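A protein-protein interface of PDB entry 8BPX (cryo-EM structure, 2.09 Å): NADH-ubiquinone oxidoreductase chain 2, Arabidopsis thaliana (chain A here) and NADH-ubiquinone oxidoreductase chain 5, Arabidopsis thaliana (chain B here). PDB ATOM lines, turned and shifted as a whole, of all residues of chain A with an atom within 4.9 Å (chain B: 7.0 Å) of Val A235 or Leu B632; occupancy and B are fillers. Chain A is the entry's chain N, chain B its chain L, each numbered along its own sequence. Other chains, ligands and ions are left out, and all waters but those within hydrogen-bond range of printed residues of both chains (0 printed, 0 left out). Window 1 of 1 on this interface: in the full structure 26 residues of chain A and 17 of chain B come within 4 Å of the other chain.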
ATOM      1  N   ILE A 189     -17.270  -7.100 -15.183  1.00  0.00           N
ATOM      2  CA  ILE A 189     -17.165  -7.882 -16.415  1.00  0.00           C
ATOM      3  C   ILE A 189     -16.296  -9.124 -16.190  1.00  0.00           C
ATOM      4  O   ILE A 189     -16.654 -10.247 -16.586  1.00  0.00           O
ATOM      5  CB  ILE A 189     -16.625  -7.001 -17.557  1.00  0.00           C
ATOM      6  CG1 ILE A 189     -17.682  -5.973 -17.974  1.00  0.00           C
ATOM      7  CG2 ILE A 189     -16.202  -7.850 -18.746  1.00  0.00           C
ATOM      8  CD1 ILE A 189     -17.136  -4.822 -18.785  1.00  0.00           C
ATOM      9  N   LEU A 231     -13.503 -14.654 -22.728  1.00  0.00           N
ATOM     10  CA  LEU A 231     -13.536 -13.322 -23.327  1.00  0.00           C
ATOM     11  C   LEU A 231     -13.705 -12.234 -22.272  1.00  0.00           C
ATOM     12  O   LEU A 231     -13.000 -11.217 -22.293  1.00  0.00           O
ATOM     13  CB  LEU A 231     -14.656 -13.225 -24.356  1.00  0.00           C
ATOM     14  CG  LEU A 231     -14.258 -13.689 -25.748  1.00  0.00           C
ATOM     15  CD1 LEU A 231     -15.491 -13.778 -26.629  1.00  0.00           C
ATOM     16  CD2 LEU A 231     -13.192 -12.781 -26.322  1.00  0.00           C
ATOM     17  N   PHE A 232     -14.646 -12.425 -21.344  1.00  0.00           N
ATOM     18  CA  PHE A 232     -14.894 -11.410 -20.324  1.00  0.00           C
ATOM     19  C   PHE A 232     -13.689 -11.249 -19.399  1.00  0.00           C
ATOM     20  O   PHE A 232     -13.319 -10.121 -19.031  1.00  0.00           O
ATOM     21  CB  PHE A 232     -16.156 -11.764 -19.533  1.00  0.00           C
ATOM     22  CG  PHE A 232     -17.442 -11.343 -20.208  1.00  0.00           C
ATOM     23  CD1 PHE A 232     -17.741 -11.762 -21.494  1.00  0.00           C
ATOM     24  CD2 PHE A 232     -18.351 -10.532 -19.550  1.00  0.00           C
ATOM     25  CE1 PHE A 232     -18.919 -11.380 -22.114  1.00  0.00           C
ATOM     26  CE2 PHE A 232     -19.534 -10.146 -20.165  1.00  0.00           C
ATOM     27  CZ  PHE A 232     -19.817 -10.572 -21.447  1.00  0.00           C
ATOM     28  N   ILE A 233     -13.059 -12.366 -19.020  1.00  0.00           N
ATOM     29  CA  ILE A 233     -11.855 -12.290 -18.198  1.00  0.00           C
ATOM     30  C   ILE A 233     -10.755 -11.539 -18.940  1.00  0.00           C
ATOM     31  O   ILE A 233     -10.036 -10.716 -18.356  1.00  0.00           O
ATOM     32  CB  ILE A 233     -11.407 -13.702 -17.775  1.00  0.00           C
ATOM     33  CG1 ILE A 233     -12.248 -14.189 -16.595  1.00  0.00           C
ATOM     34  CG2 ILE A 233      -9.925 -13.723 -17.423  1.00  0.00           C
ATOM     35  CD1 ILE A 233     -12.047 -15.639 -16.268  1.00  0.00           C
ATOM     36  N   ALA A 234     -10.617 -11.800 -20.243  1.00  0.00           N
ATOM     37  CA  ALA A 234      -9.624 -11.094 -21.043  1.00  0.00           C
ATOM     38  C   ALA A 234      -9.915  -9.601 -21.084  1.00  0.00           C
ATOM     39  O   ALA A 234      -8.992  -8.785 -21.070  1.00  0.00           O
ATOM     40  CB  ALA A 234      -9.578 -11.669 -22.458  1.00  0.00           C
ATOM     41  N   VAL A 235     -11.194  -9.229 -21.154  1.00  0.00           N
ATOM     42  CA  VAL A 235     -11.552  -7.812 -21.163  1.00  0.00           C
ATOM     43  C   VAL A 235     -11.115  -7.147 -19.865  1.00  0.00           C
ATOM     44  O   VAL A 235     -10.548  -6.045 -19.872  1.00  0.00           O
ATOM     45  CB  VAL A 235     -13.062  -7.641 -21.416  1.00  0.00           C
ATOM     46  CG1 VAL A 235     -13.517  -6.240 -21.030  1.00  0.00           C
ATOM     47  CG2 VAL A 235     -13.385  -7.920 -22.873  1.00  0.00           C
ATOM     48  N   GLY A 236     -11.360  -7.807 -18.731  1.00  0.00           N
ATOM     49  CA  GLY A 236     -10.879  -7.267 -17.466  1.00  0.00           C
ATOM     50  C   GLY A 236      -9.366  -7.118 -17.431  1.00  0.00           C
ATOM     51  O   GLY A 236      -8.830  -6.087 -17.003  1.00  0.00           O
ATOM     52  N   PHE A 237      -8.658  -8.142 -17.908  1.00  0.00           N
ATOM     53  CA  PHE A 237      -7.196  -8.102 -17.933  1.00  0.00           C
ATOM     54  C   PHE A 237      -6.689  -6.957 -18.810  1.00  0.00           C
ATOM     55  O   PHE A 237      -5.748  -6.242 -18.437  1.00  0.00           O
ATOM     56  CB  PHE A 237      -6.671  -9.444 -18.443  1.00  0.00           C
ATOM     57  CG  PHE A 237      -6.610 -10.515 -17.392  1.00  0.00           C
ATOM     58  CD1 PHE A 237      -6.913 -10.237 -16.075  1.00  0.00           C
ATOM     59  CD2 PHE A 237      -6.318 -11.820 -17.739  1.00  0.00           C
ATOM     60  CE1 PHE A 237      -6.876 -11.232 -15.115  1.00  0.00           C
ATOM     61  CE2 PHE A 237      -6.283 -12.818 -16.788  1.00  0.00           C
ATOM     62  CZ  PHE A 237      -6.563 -12.525 -15.474  1.00  0.00           C
ATOM     63  N   LEU A 238      -7.305  -6.772 -19.978  1.00  0.00           N
ATOM     64  CA  LEU A 238      -6.892  -5.720 -20.900  1.00  0.00           C
ATOM     65  C   LEU A 238      -7.162  -4.340 -20.322  1.00  0.00           C
ATOM     66  O   LEU A 238      -6.367  -3.413 -20.523  1.00  0.00           O
ATOM     67  CB  LEU A 238      -7.600  -5.886 -22.243  1.00  0.00           C
ATOM     68  CG  LEU A 238      -7.208  -7.095 -23.093  1.00  0.00           C
ATOM     69  CD1 LEU A 238      -8.305  -7.413 -24.102  1.00  0.00           C
ATOM     70  CD2 LEU A 238      -5.875  -6.859 -23.781  1.00  0.00           C
ATOM     71  N   PHE A 239      -8.285  -4.173 -19.619  1.00  0.00           N
ATOM     72  CA  PHE A 239      -8.488  -2.943 -18.862  1.00  0.00           C
ATOM     73  C   PHE A 239      -7.328  -2.717 -17.903  1.00  0.00           C
ATOM     74  O   PHE A 239      -6.785  -1.612 -17.813  1.00  0.00           O
ATOM     75  CB  PHE A 239      -9.815  -2.989 -18.100  1.00  0.00           C
ATOM     76  CG  PHE A 239     -10.059  -1.783 -17.228  1.00  0.00           C
ATOM     77  CD1 PHE A 239      -9.579  -1.733 -15.928  1.00  0.00           C
ATOM     78  CD2 PHE A 239     -10.760  -0.695 -17.714  1.00  0.00           C
ATOM     79  CE1 PHE A 239      -9.798  -0.621 -15.133  1.00  0.00           C
ATOM     80  CE2 PHE A 239     -10.988   0.416 -16.922  1.00  0.00           C
ATOM     81  CZ  PHE A 239     -10.502   0.455 -15.633  1.00  0.00           C
ATOM     82  N   PHE A 246      -9.586  -0.512 -24.015  1.00  0.00           N
ATOM     83  CA  PHE A 246      -9.946  -0.413 -22.603  1.00  0.00           C
ATOM     84  C   PHE A 246      -8.948   0.444 -21.833  1.00  0.00           C
ATOM     85  O   PHE A 246      -8.605   0.153 -20.685  1.00  0.00           O
ATOM     86  CB  PHE A 246     -10.067  -1.810 -22.005  1.00  0.00           C
ATOM     87  CG  PHE A 246     -10.832  -2.770 -22.876  1.00  0.00           C
ATOM     88  CD1 PHE A 246     -12.216  -2.777 -22.873  1.00  0.00           C
ATOM     89  CD2 PHE A 246     -10.166  -3.654 -23.709  1.00  0.00           C
ATOM     90  CE1 PHE A 246     -12.922  -3.653 -23.679  1.00  0.00           C
ATOM     91  CE2 PHE A 246     -10.866  -4.534 -24.516  1.00  0.00           C
ATOM     92  CZ  PHE A 246     -12.245  -4.533 -24.501  1.00  0.00           C
ATOM     93  N   PHE B 626     -18.667   3.936 -22.429  1.00  0.00           N
ATOM     94  CA  PHE B 626     -19.228   3.547 -23.720  1.00  0.00           C
ATOM     95  C   PHE B 626     -18.187   2.846 -24.580  1.00  0.00           C
ATOM     96  O   PHE B 626     -18.494   1.861 -25.261  1.00  0.00           O
ATOM     97  CB  PHE B 626     -19.777   4.783 -24.432  1.00  0.00           C
ATOM     98  CG  PHE B 626     -20.563   4.481 -25.680  1.00  0.00           C
ATOM     99  CD1 PHE B 626     -21.357   3.350 -25.766  1.00  0.00           C
ATOM    100  CD2 PHE B 626     -20.517   5.343 -26.764  1.00  0.00           C
ATOM    101  CE1 PHE B 626     -22.086   3.079 -26.913  1.00  0.00           C
ATOM    102  CE2 PHE B 626     -21.242   5.077 -27.916  1.00  0.00           C
ATOM    103  CZ  PHE B 626     -22.026   3.946 -27.990  1.00  0.00           C
ATOM    104  N   ALA B 627     -16.946   3.339 -24.559  1.00  0.00           N
ATOM    105  CA  ALA B 627     -15.877   2.694 -25.311  1.00  0.00           C
ATOM    106  C   ALA B 627     -15.635   1.270 -24.823  1.00  0.00           C
ATOM    107  O   ALA B 627     -15.461   0.353 -25.632  1.00  0.00           O
ATOM    108  CB  ALA B 627     -14.595   3.517 -25.211  1.00  0.00           C
ATOM    109  N   MET B 628     -15.622   1.067 -23.504  1.00  0.00           N
ATOM    110  CA  MET B 628     -15.437  -0.278 -22.969  1.00  0.00           C
ATOM    111  C   MET B 628     -16.576  -1.198 -23.387  1.00  0.00           C
ATOM    112  O   MET B 628     -16.346  -2.354 -23.763  1.00  0.00           O
ATOM    113  CB  MET B 628     -15.322  -0.227 -21.446  1.00  0.00           C
ATOM    114  CG  MET B 628     -14.050   0.423 -20.937  1.00  0.00           C
ATOM    115  SD  MET B 628     -14.201   0.932 -19.215  1.00  0.00           S
ATOM    116  CE  MET B 628     -14.227  -0.656 -18.391  1.00  0.00           C
ATOM    117  N   LEU B 629     -17.811  -0.699 -23.334  1.00  0.00           N
ATOM    118  CA  LEU B 629     -18.954  -1.483 -23.790  1.00  0.00           C
ATOM    119  C   LEU B 629     -18.841  -1.808 -25.274  1.00  0.00           C
ATOM    120  O   LEU B 629     -19.100  -2.941 -25.691  1.00  0.00           O
ATOM    121  CB  LEU B 629     -20.247  -0.721 -23.503  1.00  0.00           C
ATOM    122  CG  LEU B 629     -21.584  -1.408 -23.780  1.00  0.00           C
ATOM    123  CD1 LEU B 629     -21.564  -2.863 -23.339  1.00  0.00           C
ATOM    124  CD2 LEU B 629     -22.709  -0.646 -23.099  1.00  0.00           C
ATOM    125  N   LEU B 630     -18.445  -0.823 -26.084  1.00  0.00           N
ATOM    126  CA  LEU B 630     -18.287  -1.056 -27.515  1.00  0.00           C
ATOM    127  C   LEU B 630     -17.201  -2.090 -27.789  1.00  0.00           C
ATOM    128  O   LEU B 630     -17.369  -2.964 -28.647  1.00  0.00           O
ATOM    129  CB  LEU B 630     -17.969   0.259 -28.221  1.00  0.00           C
ATOM    130  CG  LEU B 630     -19.152   1.192 -28.489  1.00  0.00           C
ATOM    131  CD1 LEU B 630     -18.682   2.455 -29.194  1.00  0.00           C
ATOM    132  CD2 LEU B 630     -20.240   0.494 -29.295  1.00  0.00           C
ATOM    133  N   GLY B 631     -16.079  -2.003 -27.073  1.00  0.00           N
ATOM    134  CA  GLY B 631     -15.033  -2.997 -27.234  1.00  0.00           C
ATOM    135  C   GLY B 631     -15.486  -4.389 -26.835  1.00  0.00           C
ATOM    136  O   GLY B 631     -15.160  -5.373 -27.502  1.00  0.00           O
ATOM    137  N   LEU B 632     -16.241  -4.487 -25.740  1.00  0.00           N
ATOM    138  CA  LEU B 632     -16.800  -5.775 -25.339  1.00  0.00           C
ATOM    139  C   LEU B 632     -17.771  -6.307 -26.388  1.00  0.00           C
ATOM    140  O   LEU B 632     -17.744  -7.496 -26.725  1.00  0.00           O
ATOM    141  CB  LEU B 632     -17.489  -5.641 -23.982  1.00  0.00           C
ATOM    142  CG  LEU B 632     -18.201  -6.870 -23.422  1.00  0.00           C
ATOM    143  CD1 LEU B 632     -17.200  -7.959 -23.074  1.00  0.00           C
ATOM    144  CD2 LEU B 632     -19.027  -6.496 -22.206  1.00  0.00           C
ATOM    145  N   THR B 633     -18.630  -5.437 -26.923  1.00  0.00           N
ATOM    146  CA  THR B 633     -19.569  -5.857 -27.960  1.00  0.00           C
ATOM    147  C   THR B 633     -18.841  -6.303 -29.220  1.00  0.00           C
ATOM    148  O   THR B 633     -19.199  -7.319 -29.827  1.00  0.00           O
ATOM    149  CB  THR B 633     -20.538  -4.718 -28.278  1.00  0.00           C
ATOM    150  OG1 THR B 633     -21.168  -4.278 -27.070  1.00  0.00           O
ATOM    151  CG2 THR B 633     -21.598  -5.179 -29.266  1.00  0.00           C
ATOM    152  N   LEU B 634     -17.845  -5.530 -29.644  1.00  0.00           N
ATOM    153  CA  LEU B 634     -16.987  -5.906 -30.791  1.00  0.00           C
ATOM    154  C   LEU B 634     -16.390  -7.300 -30.549  1.00  0.00           C
ATOM    155  O   LEU B 634     -16.448  -8.123 -31.476  1.00  0.00           O
ATOM    156  CB  LEU B 634     -15.898  -4.841 -30.964  1.00  0.00           C
ATOM    157  CG  LEU B 634     -14.736  -5.228 -31.877  1.00  0.00           C
ATOM    158  CD1 LEU B 634     -15.141  -5.132 -33.339  1.00  0.00           C
ATOM    159  CD2 LEU B 634     -13.518  -4.361 -31.598  1.00  0.00           C
ATOM    160  N   PHE B 635     -15.847  -7.545 -29.357  1.00  0.00           N
ATOM    161  CA  PHE B 635     -15.213  -8.822 -29.046  1.00  0.00           C
ATOM    162  C   PHE B 635     -16.177  -9.983 -29.254  1.00  0.00           C
ATOM    163  O   PHE B 635     -15.862 -10.955 -29.950  1.00  0.00           O
ATOM    164  CB  PHE B 635     -14.705  -8.811 -27.607  1.00  0.00           C
ATOM    165  CG  PHE B 635     -13.301  -8.313 -27.458  1.00  0.00           C
ATOM    166  CD1 PHE B 635     -12.699  -7.574 -28.462  1.00  0.00           C
ATOM    167  CD2 PHE B 635     -12.585  -8.576 -26.305  1.00  0.00           C
ATOM    168  CE1 PHE B 635     -11.404  -7.108 -28.316  1.00  0.00           C
ATOM    169  CE2 PHE B 635     -11.291  -8.117 -26.155  1.00  0.00           C
ATOM    170  CZ  PHE B 635     -10.702  -7.381 -27.160  1.00  0.00           C
ATOM    171  N   VAL B 636     -17.364  -9.892 -28.652  1.00  0.00           N
ATOM    172  CA  VAL B 636     -18.363 -10.949 -28.792  1.00  0.00           C
ATOM    173  C   VAL B 636     -18.771 -11.101 -30.250  1.00  0.00           C
ATOM    174  O   VAL B 636     -18.849 -12.216 -30.779  1.00  0.00           O
ATOM    175  CB  VAL B 636     -19.577 -10.653 -27.894  1.00  0.00           C
ATOM    176  CG1 VAL B 636     -20.716 -11.618 -28.197  1.00  0.00           C
ATOM    177  CG2 VAL B 636     -19.181 -10.732 -26.431  1.00  0.00           C
ATOM    178  N   THR B 637     -19.020  -9.980 -30.925  1.00  0.00           N
ATOM    179  CA  THR B 637     -19.548 -10.031 -32.284  1.00  0.00           C
ATOM    180  C   THR B 637     -18.560 -10.681 -33.242  1.00  0.00           C
ATOM    181  O   THR B 637     -18.904 -11.631 -33.955  1.00  0.00           O
ATOM    182  CB  THR B 637     -19.911  -8.624 -32.758  1.00  0.00           C
ATOM    183  OG1 THR B 637     -21.203  -8.273 -32.250  1.00  0.00           O
ATOM    184  CG2 THR B 637     -19.938  -8.561 -34.280  1.00  0.00           C
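Among the printed residues, pairs that only touch across the chains: Phe A232 with Leu B632, Val A235 with Leu B632, Val A235 with Phe B635, Leu A238 with Phe B635, Phe A239 with Met B628, Phe A246 with Met B628, Phe A246 with Gly B631, Phe A246 with Leu B632 and Phe A246 with Phe B635.
Of the 12 printed residues of chain B, 4 touch a printed residue of chain A. Hydrophobic or aromatic side chains of chain B that line the printed part of chain A: Met B628, Leu B632 and Phe B635. Among the printed residues, no Asp or Glu carboxylate lies within 4 Å of a Lys or Arg side-chain nitrogen of the other chain.
Of chain B, only Leu B632 (3.8 Å) and Phe B635 (3.6 Å) come within 4 Å of Val A235. Printed residues of chain A within 4 Å of Leu B632: Phe A232 (3.9 Å), Val A235 (3.8 Å) and Phe A246 (3.99 Å). Of the printed residues of chain B, Phe A239 touches Met B628. Printed residues of chain A within 4 Å of Phe B635: Val A235 (3.6 Å), Leu A238 (3.7 Å) and Phe A246 (3.9 Å). Printed residues of chain B within 4 Å of Phe A232: Leu B632 (3.9 Å). Ile A233 touches none of the printed residues of chain B. Ala B627 touches none of the printed residues of chain A.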
